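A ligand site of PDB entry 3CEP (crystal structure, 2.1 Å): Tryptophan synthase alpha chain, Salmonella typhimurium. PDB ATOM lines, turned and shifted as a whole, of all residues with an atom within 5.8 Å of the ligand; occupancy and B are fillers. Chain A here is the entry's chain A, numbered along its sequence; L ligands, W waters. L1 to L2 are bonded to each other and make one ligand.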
ATOM      1  N   PHE A  22      25.066 -12.799 -29.462  1.00  0.00           N
ATOM      2  CA  PHE A  22      25.813 -12.007 -28.466  1.00  0.00           C
ATOM      3  C   PHE A  22      27.043 -12.757 -27.953  1.00  0.00           C
ATOM      4  O   PHE A  22      26.995 -13.963 -27.726  1.00  0.00           O
ATOM      5  CB  PHE A  22      24.922 -11.604 -27.282  1.00  0.00           C
ATOM      6  CG  PHE A  22      25.704 -11.160 -26.060  1.00  0.00           C
ATOM      7  CD1 PHE A  22      26.085 -12.095 -25.086  1.00  0.00           C
ATOM      8  CD2 PHE A  22      26.064  -9.842 -25.895  1.00  0.00           C
ATOM      9  CE1 PHE A  22      26.817 -11.697 -23.964  1.00  0.00           C
ATOM     10  CE2 PHE A  22      26.796  -9.430 -24.772  1.00  0.00           C
ATOM     11  CZ  PHE A  22      27.173 -10.365 -23.807  1.00  0.00           C
ATOM     12  N   GLU A  49      25.698  -8.158 -31.063  1.00  0.00           N
ATOM     13  CA  GLU A  49      25.594  -7.582 -29.737  1.00  0.00           C
ATOM     14  C   GLU A  49      26.826  -8.017 -28.943  1.00  0.00           C
ATOM     15  O   GLU A  49      27.107  -9.204 -28.826  1.00  0.00           O
ATOM     16  CB  GLU A  49      24.289  -7.984 -29.030  1.00  0.00           C
ATOM     17  CG  GLU A  49      24.038  -7.211 -27.742  1.00  0.00           C
ATOM     18  CD  GLU A  49      23.014  -7.898 -26.838  1.00  0.00           C
ATOM     19  OE1 GLU A  49      23.170  -7.793 -25.594  1.00  0.00           O
ATOM     20  OE2 GLU A  49      22.082  -8.542 -27.357  1.00  0.00           O
ATOM     21  N   ALA A  59      21.585  -8.502 -14.643  1.00  0.00           N
ATOM     22  CA  ALA A  59      20.567  -9.056 -15.548  1.00  0.00           C
ATOM     23  C   ALA A  59      21.009 -10.374 -16.193  1.00  0.00           C
ATOM     24  O   ALA A  59      20.379 -10.862 -17.122  1.00  0.00           O
ATOM     25  CB  ALA A  59      20.161  -8.019 -16.607  1.00  0.00           C
ATOM     26  N   ASP A  60      22.073 -10.973 -15.657  1.00  0.00           N
ATOM     27  CA  ASP A  60      22.691 -12.132 -16.275  1.00  0.00           C
ATOM     28  C   ASP A  60      22.709 -13.369 -15.381  1.00  0.00           C
ATOM     29  O   ASP A  60      23.026 -13.287 -14.197  1.00  0.00           O
ATOM     30  CB  ASP A  60      24.115 -11.800 -16.731  1.00  0.00           C
ATOM     31  CG  ASP A  60      24.125 -10.993 -18.009  1.00  0.00           C
ATOM     32  OD1 ASP A  60      23.663 -11.523 -19.035  1.00  0.00           O
ATOM     33  OD2 ASP A  60      24.606  -9.830 -17.988  1.00  0.00           O
ATOM     34  N   ILE A  64      26.506 -16.220 -18.779  1.00  0.00           N
ATOM     35  CA  ILE A  64      27.139 -14.948 -19.126  1.00  0.00           C
ATOM     36  C   ILE A  64      27.941 -14.373 -17.953  1.00  0.00           C
ATOM     37  O   ILE A  64      28.956 -13.699 -18.167  1.00  0.00           O
ATOM     38  CB  ILE A  64      26.128 -13.935 -19.716  1.00  0.00           C
ATOM     39  CG1 ILE A  64      25.610 -14.447 -21.065  1.00  0.00           C
ATOM     40  CG2 ILE A  64      26.787 -12.590 -19.909  1.00  0.00           C
ATOM     41  CD1 ILE A  64      24.447 -13.657 -21.650  1.00  0.00           C
ATOM     42  N   LEU A 100      26.149  -4.121 -25.156  1.00  0.00           N
ATOM     43  CA  LEU A 100      25.378  -4.333 -23.945  1.00  0.00           C
ATOM     44  C   LEU A 100      26.221  -3.828 -22.791  1.00  0.00           C
ATOM     45  O   LEU A 100      27.311  -4.352 -22.527  1.00  0.00           O
ATOM     46  CB  LEU A 100      24.990  -5.800 -23.742  1.00  0.00           C
ATOM     47  CG  LEU A 100      24.051  -6.135 -22.559  1.00  0.00           C
ATOM     48  CD1 LEU A 100      24.772  -6.215 -21.184  1.00  0.00           C
ATOM     49  CD2 LEU A 100      22.877  -5.172 -22.513  1.00  0.00           C
ATOM     50  N   TYR A 102      26.294  -2.096 -18.639  1.00  0.00           N
ATOM     51  CA  TYR A 102      25.682  -1.762 -17.350  1.00  0.00           C
ATOM     52  C   TYR A 102      25.973  -0.288 -17.063  1.00  0.00           C
ATOM     53  O   TYR A 102      27.000   0.233 -17.494  1.00  0.00           O
ATOM     54  CB  TYR A 102      26.163  -2.693 -16.233  1.00  0.00           C
ATOM     55  CG  TYR A 102      25.473  -4.035 -16.344  1.00  0.00           C
ATOM     56  CD1 TYR A 102      24.240  -4.262 -15.739  1.00  0.00           C
ATOM     57  CD2 TYR A 102      26.027  -5.069 -17.115  1.00  0.00           C
ATOM     58  CE1 TYR A 102      23.575  -5.468 -15.867  1.00  0.00           C
ATOM     59  CE2 TYR A 102      25.369  -6.296 -17.247  1.00  0.00           C
ATOM     60  CZ  TYR A 102      24.154  -6.488 -16.616  1.00  0.00           C
ATOM     61  OH  TYR A 102      23.500  -7.701 -16.738  1.00  0.00           O
ATOM     62  N   LEU A 127      22.774  -0.681 -25.435  1.00  0.00           N
ATOM     63  CA  LEU A 127      21.731  -1.114 -24.515  1.00  0.00           C
ATOM     64  C   LEU A 127      22.294  -1.028 -23.100  1.00  0.00           C
ATOM     65  O   LEU A 127      23.271  -1.698 -22.790  1.00  0.00           O
ATOM     66  CB  LEU A 127      21.311  -2.548 -24.811  1.00  0.00           C
ATOM     67  CG  LEU A 127      19.903  -3.078 -24.531  1.00  0.00           C
ATOM     68  CD1 LEU A 127      19.926  -4.602 -24.454  1.00  0.00           C
ATOM     69  CD2 LEU A 127      19.226  -2.483 -23.282  1.00  0.00           C
ATOM     70  N   ALA A 129      21.469  -2.150 -19.601  1.00  0.00           N
ATOM     71  CA  ALA A 129      20.574  -3.142 -18.979  1.00  0.00           C
ATOM     72  C   ALA A 129      19.822  -2.647 -17.733  1.00  0.00           C
ATOM     73  O   ALA A 129      18.662  -3.006 -17.524  1.00  0.00           O
ATOM     74  CB  ALA A 129      21.362  -4.411 -18.660  1.00  0.00           C
ATOM     75  N   ILE A 153      14.476  -1.892 -23.658  1.00  0.00           N
ATOM     76  CA  ILE A 153      13.788  -3.165 -23.527  1.00  0.00           C
ATOM     77  C   ILE A 153      12.290  -2.963 -23.372  1.00  0.00           C
ATOM     78  O   ILE A 153      11.833  -2.140 -22.572  1.00  0.00           O
ATOM     79  CB  ILE A 153      14.341  -3.984 -22.340  1.00  0.00           C
ATOM     80  CG1 ILE A 153      15.772  -4.451 -22.636  1.00  0.00           C
ATOM     81  CG2 ILE A 153      13.445  -5.183 -22.040  1.00  0.00           C
ATOM     82  CD1 ILE A 153      16.517  -4.991 -21.427  1.00  0.00           C
ATOM     83  N   TYR A 175      14.309  -3.762 -28.165  1.00  0.00           N
ATOM     84  CA  TYR A 175      14.628  -5.032 -27.522  1.00  0.00           C
ATOM     85  C   TYR A 175      13.360  -5.614 -26.923  1.00  0.00           C
ATOM     86  O   TYR A 175      12.825  -5.104 -25.924  1.00  0.00           O
ATOM     87  CB  TYR A 175      15.708  -4.880 -26.438  1.00  0.00           C
ATOM     88  CG  TYR A 175      16.354  -6.199 -26.025  1.00  0.00           C
ATOM     89  CD1 TYR A 175      15.629  -7.168 -25.346  1.00  0.00           C
ATOM     90  CD2 TYR A 175      17.700  -6.455 -26.322  1.00  0.00           C
ATOM     91  CE1 TYR A 175      16.216  -8.380 -24.971  1.00  0.00           C
ATOM     92  CE2 TYR A 175      18.297  -7.660 -25.940  1.00  0.00           C
ATOM     93  CZ  TYR A 175      17.551  -8.615 -25.273  1.00  0.00           C
ATOM     94  OH  TYR A 175      18.144  -9.805 -24.900  1.00  0.00           O
ATOM     95  N   ARG A 179      10.737 -12.924 -21.787  1.00  0.00           N
ATOM     96  CA  ARG A 179      10.299 -13.396 -20.454  1.00  0.00           C
ATOM     97  C   ARG A 179      10.955 -12.574 -19.363  1.00  0.00           C
ATOM     98  O   ARG A 179      11.969 -11.906 -19.598  1.00  0.00           O
ATOM     99  CB  ARG A 179      10.670 -14.875 -20.244  1.00  0.00           C
ATOM    100  CG  ARG A 179      12.157 -15.202 -20.473  1.00  0.00           C
ATOM    101  CD  ARG A 179      12.635 -16.357 -19.612  1.00  0.00           C
ATOM    102  NE  ARG A 179      14.020 -16.718 -19.918  1.00  0.00           N
ATOM    103  CZ  ARG A 179      15.094 -16.171 -19.365  1.00  0.00           C
ATOM    104  NH1 ARG A 179      14.974 -15.225 -18.436  1.00  0.00           N
ATOM    105  NH2 ARG A 179      16.309 -16.569 -19.729  1.00  0.00           N
ATOM    106  N   VAL A 182      16.476 -13.443 -15.699  1.00  0.00           N
ATOM    107  CA  VAL A 182      17.791 -13.035 -16.170  1.00  0.00           C
ATOM    108  C   VAL A 182      18.179 -13.887 -17.378  1.00  0.00           C
ATOM    109  O   VAL A 182      17.503 -14.859 -17.690  1.00  0.00           O
ATOM    110  CB  VAL A 182      18.879 -13.139 -15.054  1.00  0.00           C
ATOM    111  CG1 VAL A 182      18.524 -12.244 -13.870  1.00  0.00           C
ATOM    112  CG2 VAL A 182      19.073 -14.583 -14.591  1.00  0.00           C
ATOM    113  N   THR A 183      19.260 -13.511 -18.054  1.00  0.00           N
ATOM    114  CA  THR A 183      19.689 -14.234 -19.264  1.00  0.00           C
ATOM    115  C   THR A 183      19.923 -15.713 -18.961  1.00  0.00           C
ATOM    116  O   THR A 183      20.339 -16.072 -17.855  1.00  0.00           O
ATOM    117  CB  THR A 183      20.968 -13.616 -19.889  1.00  0.00           C
ATOM    118  OG1 THR A 183      22.064 -13.741 -18.972  1.00  0.00           O
ATOM    119  CG2 THR A 183      20.751 -12.156 -20.243  1.00  0.00           C
ATOM    120  N   GLY A 184      19.633 -16.567 -19.940  1.00  0.00           N
ATOM    121  CA  GLY A 184      19.794 -17.999 -19.767  1.00  0.00           C
ATOM    122  C   GLY A 184      19.167 -18.791 -20.892  1.00  0.00           C
ATOM    123  O   GLY A 184      17.974 -18.636 -21.177  1.00  0.00           O
ATOM    124  N   ALA A 185      19.971 -19.634 -21.516  1.00  0.00           N
ATOM    125  CA  ALA A 185      19.550 -20.478 -22.634  1.00  0.00           C
ATOM    126  C   ALA A 185      18.525 -21.557 -22.231  1.00  0.00           C
ATOM    127  O   ALA A 185      17.684 -21.955 -23.033  1.00  0.00           O
ATOM    128  CB  ALA A 185      20.760 -21.127 -23.298  1.00  0.00           C
ATOM    129  N   GLY A 211      14.772 -11.337 -27.483  1.00  0.00           N
ATOM    130  CA  GLY A 211      15.943 -11.842 -26.762  1.00  0.00           C
ATOM    131  C   GLY A 211      15.600 -12.348 -25.374  1.00  0.00           C
ATOM    132  O   GLY A 211      14.635 -11.870 -24.745  1.00  0.00           O
ATOM    133  N   PHE A 212      16.424 -13.297 -24.908  1.00  0.00           N
ATOM    134  CA  PHE A 212      16.279 -14.056 -23.635  1.00  0.00           C
ATOM    135  C   PHE A 212      15.742 -15.453 -23.879  1.00  0.00           C
ATOM    136  O   PHE A 212      14.575 -15.635 -24.239  1.00  0.00           O
ATOM    137  CB  PHE A 212      15.429 -13.337 -22.580  1.00  0.00           C
ATOM    138  CG  PHE A 212      16.190 -12.369 -21.716  1.00  0.00           C
ATOM    139  CD1 PHE A 212      16.992 -11.375 -22.286  1.00  0.00           C
ATOM    140  CD2 PHE A 212      16.072 -12.418 -20.336  1.00  0.00           C
ATOM    141  CE1 PHE A 212      17.673 -10.484 -21.487  1.00  0.00           C
ATOM    142  CE2 PHE A 212      16.753 -11.528 -19.537  1.00  0.00           C
ATOM    143  CZ  PHE A 212      17.549 -10.554 -20.105  1.00  0.00           C
ATOM    144  N   GLY A 213      16.602 -16.461 -23.692  1.00  0.00           N
ATOM    145  CA  GLY A 213      16.203 -17.852 -23.810  1.00  0.00           C
ATOM    146  C   GLY A 213      16.077 -18.424 -25.222  1.00  0.00           C
ATOM    147  O   GLY A 213      15.584 -19.532 -25.389  1.00  0.00           O
ATOM    148  N   ILE A 214      16.531 -17.674 -26.226  1.00  0.00           N
ATOM    149  CA  ILE A 214      16.514 -18.153 -27.607  1.00  0.00           C
ATOM    150  C   ILE A 214      17.770 -18.986 -27.860  1.00  0.00           C
ATOM    151  O   ILE A 214      18.882 -18.452 -27.880  1.00  0.00           O
ATOM    152  CB  ILE A 214      16.455 -16.982 -28.638  1.00  0.00           C
ATOM    153  CG1 ILE A 214      15.382 -15.937 -28.262  1.00  0.00           C
ATOM    154  CG2 ILE A 214      16.272 -17.512 -30.068  1.00  0.00           C
ATOM    155  CD1 ILE A 214      13.956 -16.443 -28.236  1.00  0.00           C
ATOM    156  N   ILE A 232      17.636 -12.661 -31.010  1.00  0.00           N
ATOM    157  CA  ILE A 232      18.948 -12.521 -30.408  1.00  0.00           C
ATOM    158  C   ILE A 232      19.234 -13.744 -29.554  1.00  0.00           C
ATOM    159  O   ILE A 232      18.393 -14.161 -28.754  1.00  0.00           O
ATOM    160  CB  ILE A 232      19.035 -11.244 -29.505  1.00  0.00           C
ATOM    161  CG1 ILE A 232      18.644  -9.985 -30.280  1.00  0.00           C
ATOM    162  CG2 ILE A 232      20.449 -11.087 -28.914  1.00  0.00           C
ATOM    163  CD1 ILE A 232      18.235  -8.831 -29.393  1.00  0.00           C
ATOM    164  N   SER A 233      20.408 -14.334 -29.742  1.00  0.00           N
ATOM    165  CA  SER A 233      20.850 -15.439 -28.908  1.00  0.00           C
ATOM    166  C   SER A 233      22.178 -15.082 -28.231  1.00  0.00           C
ATOM    167  O   SER A 233      23.149 -14.737 -28.915  1.00  0.00           O
ATOM    168  CB  SER A 233      21.008 -16.713 -29.744  1.00  0.00           C
ATOM    169  OG  SER A 233      21.420 -17.803 -28.940  1.00  0.00           O
ATOM    170  N   GLY A 234      22.191 -15.154 -26.908  1.00  0.00           N
ATOM    171  CA  GLY A 234      23.384 -14.846 -26.119  1.00  0.00           C
ATOM    172  C   GLY A 234      23.963 -16.064 -25.424  1.00  0.00           C
ATOM    173  O   GLY A 234      24.992 -16.598 -25.854  1.00  0.00           O
ATOM    174  N   SER A 235      23.298 -16.515 -24.364  1.00  0.00           N
ATOM    175  CA  SER A 235      23.783 -17.619 -23.537  1.00  0.00           C
ATOM    176  C   SER A 235      24.087 -18.898 -24.339  1.00  0.00           C
ATOM    177  O   SER A 235      25.066 -19.589 -24.042  1.00  0.00           O
ATOM    178  CB  SER A 235      22.803 -17.918 -22.390  1.00  0.00           C
ATOM    179  OG  SER A 235      22.646 -16.793 -21.548  1.00  0.00           O
ATOM    180  N   ALA A 236      23.262 -19.175 -25.341  1.00  0.00           N
ATOM    181  CA  ALA A 236      23.473 -20.325 -26.240  1.00  0.00           C
ATOM    182  C   ALA A 236      24.827 -20.248 -26.934  1.00  0.00           C
ATOM    183  O   ALA A 236      25.549 -21.235 -26.992  1.00  0.00           O
ATOM    184  CB  ALA A 236      22.355 -20.410 -27.262  1.00  0.00           C
HETATM  185  O1  LIG L   1      21.038 -10.138 -25.653  1.00  0.00           O
HETATM  186  C1  LIG L   1      21.266 -10.443 -24.386  1.00  0.00           C
HETATM  187  C2  LIG L   1      21.308 -11.902 -24.152  1.00  0.00           C
HETATM  188  O2  LIG L   1      22.263 -12.323 -23.336  1.00  0.00           O
HETATM  189  C3  LIG L   1      20.053 -12.396 -23.622  1.00  0.00           C
HETATM  190  O3  LIG L   1      19.650 -13.603 -24.322  1.00  0.00           O
HETATM  191  O4  LIG L   1      19.168 -15.328 -22.614  1.00  0.00           O
HETATM  192  O5  LIG L   1      21.576 -14.821 -23.186  1.00  0.00           O
HETATM  193  O6  LIG L   1      20.081 -15.900 -24.902  1.00  0.00           O
HETATM  194  P1  LIG L   1      20.162 -15.003 -23.690  1.00  0.00           P
HETATM  195  N1  LG2 L   2      22.278  -9.495 -23.817  1.00  0.00           N
HETATM  196  C1  LG2 L   2      23.513 -10.085 -23.225  1.00  0.00           C
HETATM  197  C2  LG2 L   2      23.512  -9.825 -21.690  1.00  0.00           C
HETATM  198  C3  LG2 L   2      22.249  -9.023 -21.544  1.00  0.00           C
HETATM  199  C4  LG2 L   2      21.734  -8.477 -20.389  1.00  0.00           C
HETATM  200  C5  LG2 L   2      20.529  -7.742 -20.488  1.00  0.00           C
HETATM  201  C6  LG2 L   2      19.878  -7.582 -21.728  1.00  0.00           C
HETATM  202  C7  LG2 L   2      20.420  -8.141 -22.895  1.00  0.00           C
HETATM  203  C8  LG2 L   2      21.615  -8.862 -22.780  1.00  0.00           C
HETATM  204  O   HOH W   1      18.023 -14.822 -26.301  1.00  0.00           O
HETATM  205  O   HOH W   2      20.487 -18.423 -25.489  1.00  0.00           O
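O1 of LIG L1 lies within hydrogen-bond range of OH of Tyr 175, at 3.0 Å. The backbone NH (N) of Phe 212 is in hydrogen-bond range of an oxygen (O3) of LIG L1 (3.3 Å). O1 of LIG L1 lies within hydrogen-bond range of OE2 of Glu 49. An oxygen (O5) of LIG L1 is in hydrogen-bond range of the backbone NH (N) of Ser 235 (2.7 Å). N of Gly 234 is in hydrogen-bond range of O6 of LIG L1, at 3.0 Å. The backbone NH of Gly 213 sits at hydrogen-bond distance from an oxygen (O4) of LIG L1, at 3.0 Å. O4 of LIG L1 sits at hydrogen-bond distance from N of Gly 184 (3.0 Å). O5 of LIG L1 sits at hydrogen-bond distance from OG of Ser 235, at 2.8 Å.
Residues that only touch the ligand: Phe 22 (3.7 Å), Ala 59 (3.9 Å), Asp 60 (3.2 Å), Ile 64 (3.1 Å), Leu 100 (3.6 Å), Leu 127 (3.9 Å), Ala 129 (3.9 Å), Thr 183 (3.4 Å) and Ile 232 (3.4 Å). Hydrophobic or aromatic side chains that line the ligand: Phe 22, Ala 59, Ile 64, Leu 100, Leu 127, Ala 129, Tyr 175, Phe 212 and Ile 232. 16 residues have an atom within 4 Å of the ligand: Phe 22, Glu 49, Ala 59, Asp 60, Ile 64, Leu 100, Leu 127, Ala 129, Tyr 175, Thr 183, Gly 184, Phe 212, Gly 213, Ile 232, Gly 234 and Ser 235. The nearest printed residue that does not touch the ligand is Ser 233 (4.02 Å).
Water W2 lies within hydrogen-bond range of an oxygen (O6) of LIG L1 (2.6 Å), the backbone carbonyl oxygen of Ile 214 (2.9 Å) and the backbone NH of Ala 236 (2.9 Å).
The backbone NH of Phe 22 is in hydrogen-bond range of the backbone carbonyl oxygen of Ser 233 (2.8 Å). N of Ala 59 sits at hydrogen-bond distance from OH of Tyr 102 (2.9 Å). O of Gly 184 is in hydrogen-bond range of NH2 of Arg 179, 3.0 Å away. OD2 of Asp 60 sits at hydrogen-bond distance from OH of Tyr 102, 2.7 Å away. OG of Ser 235 is in hydrogen-bond range of N of Gly 184 (3.4 Å). The side-chain carboxylate (OD1) of Asp 60 is in hydrogen-bond range of the side-chain hydroxyl (OG1) of Thr 183 (2.7 Å). The backbone NH (N) of Thr 183 is in hydrogen-bond range of the backbone carbonyl oxygen (O) of Ala 59 (3.0 Å).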
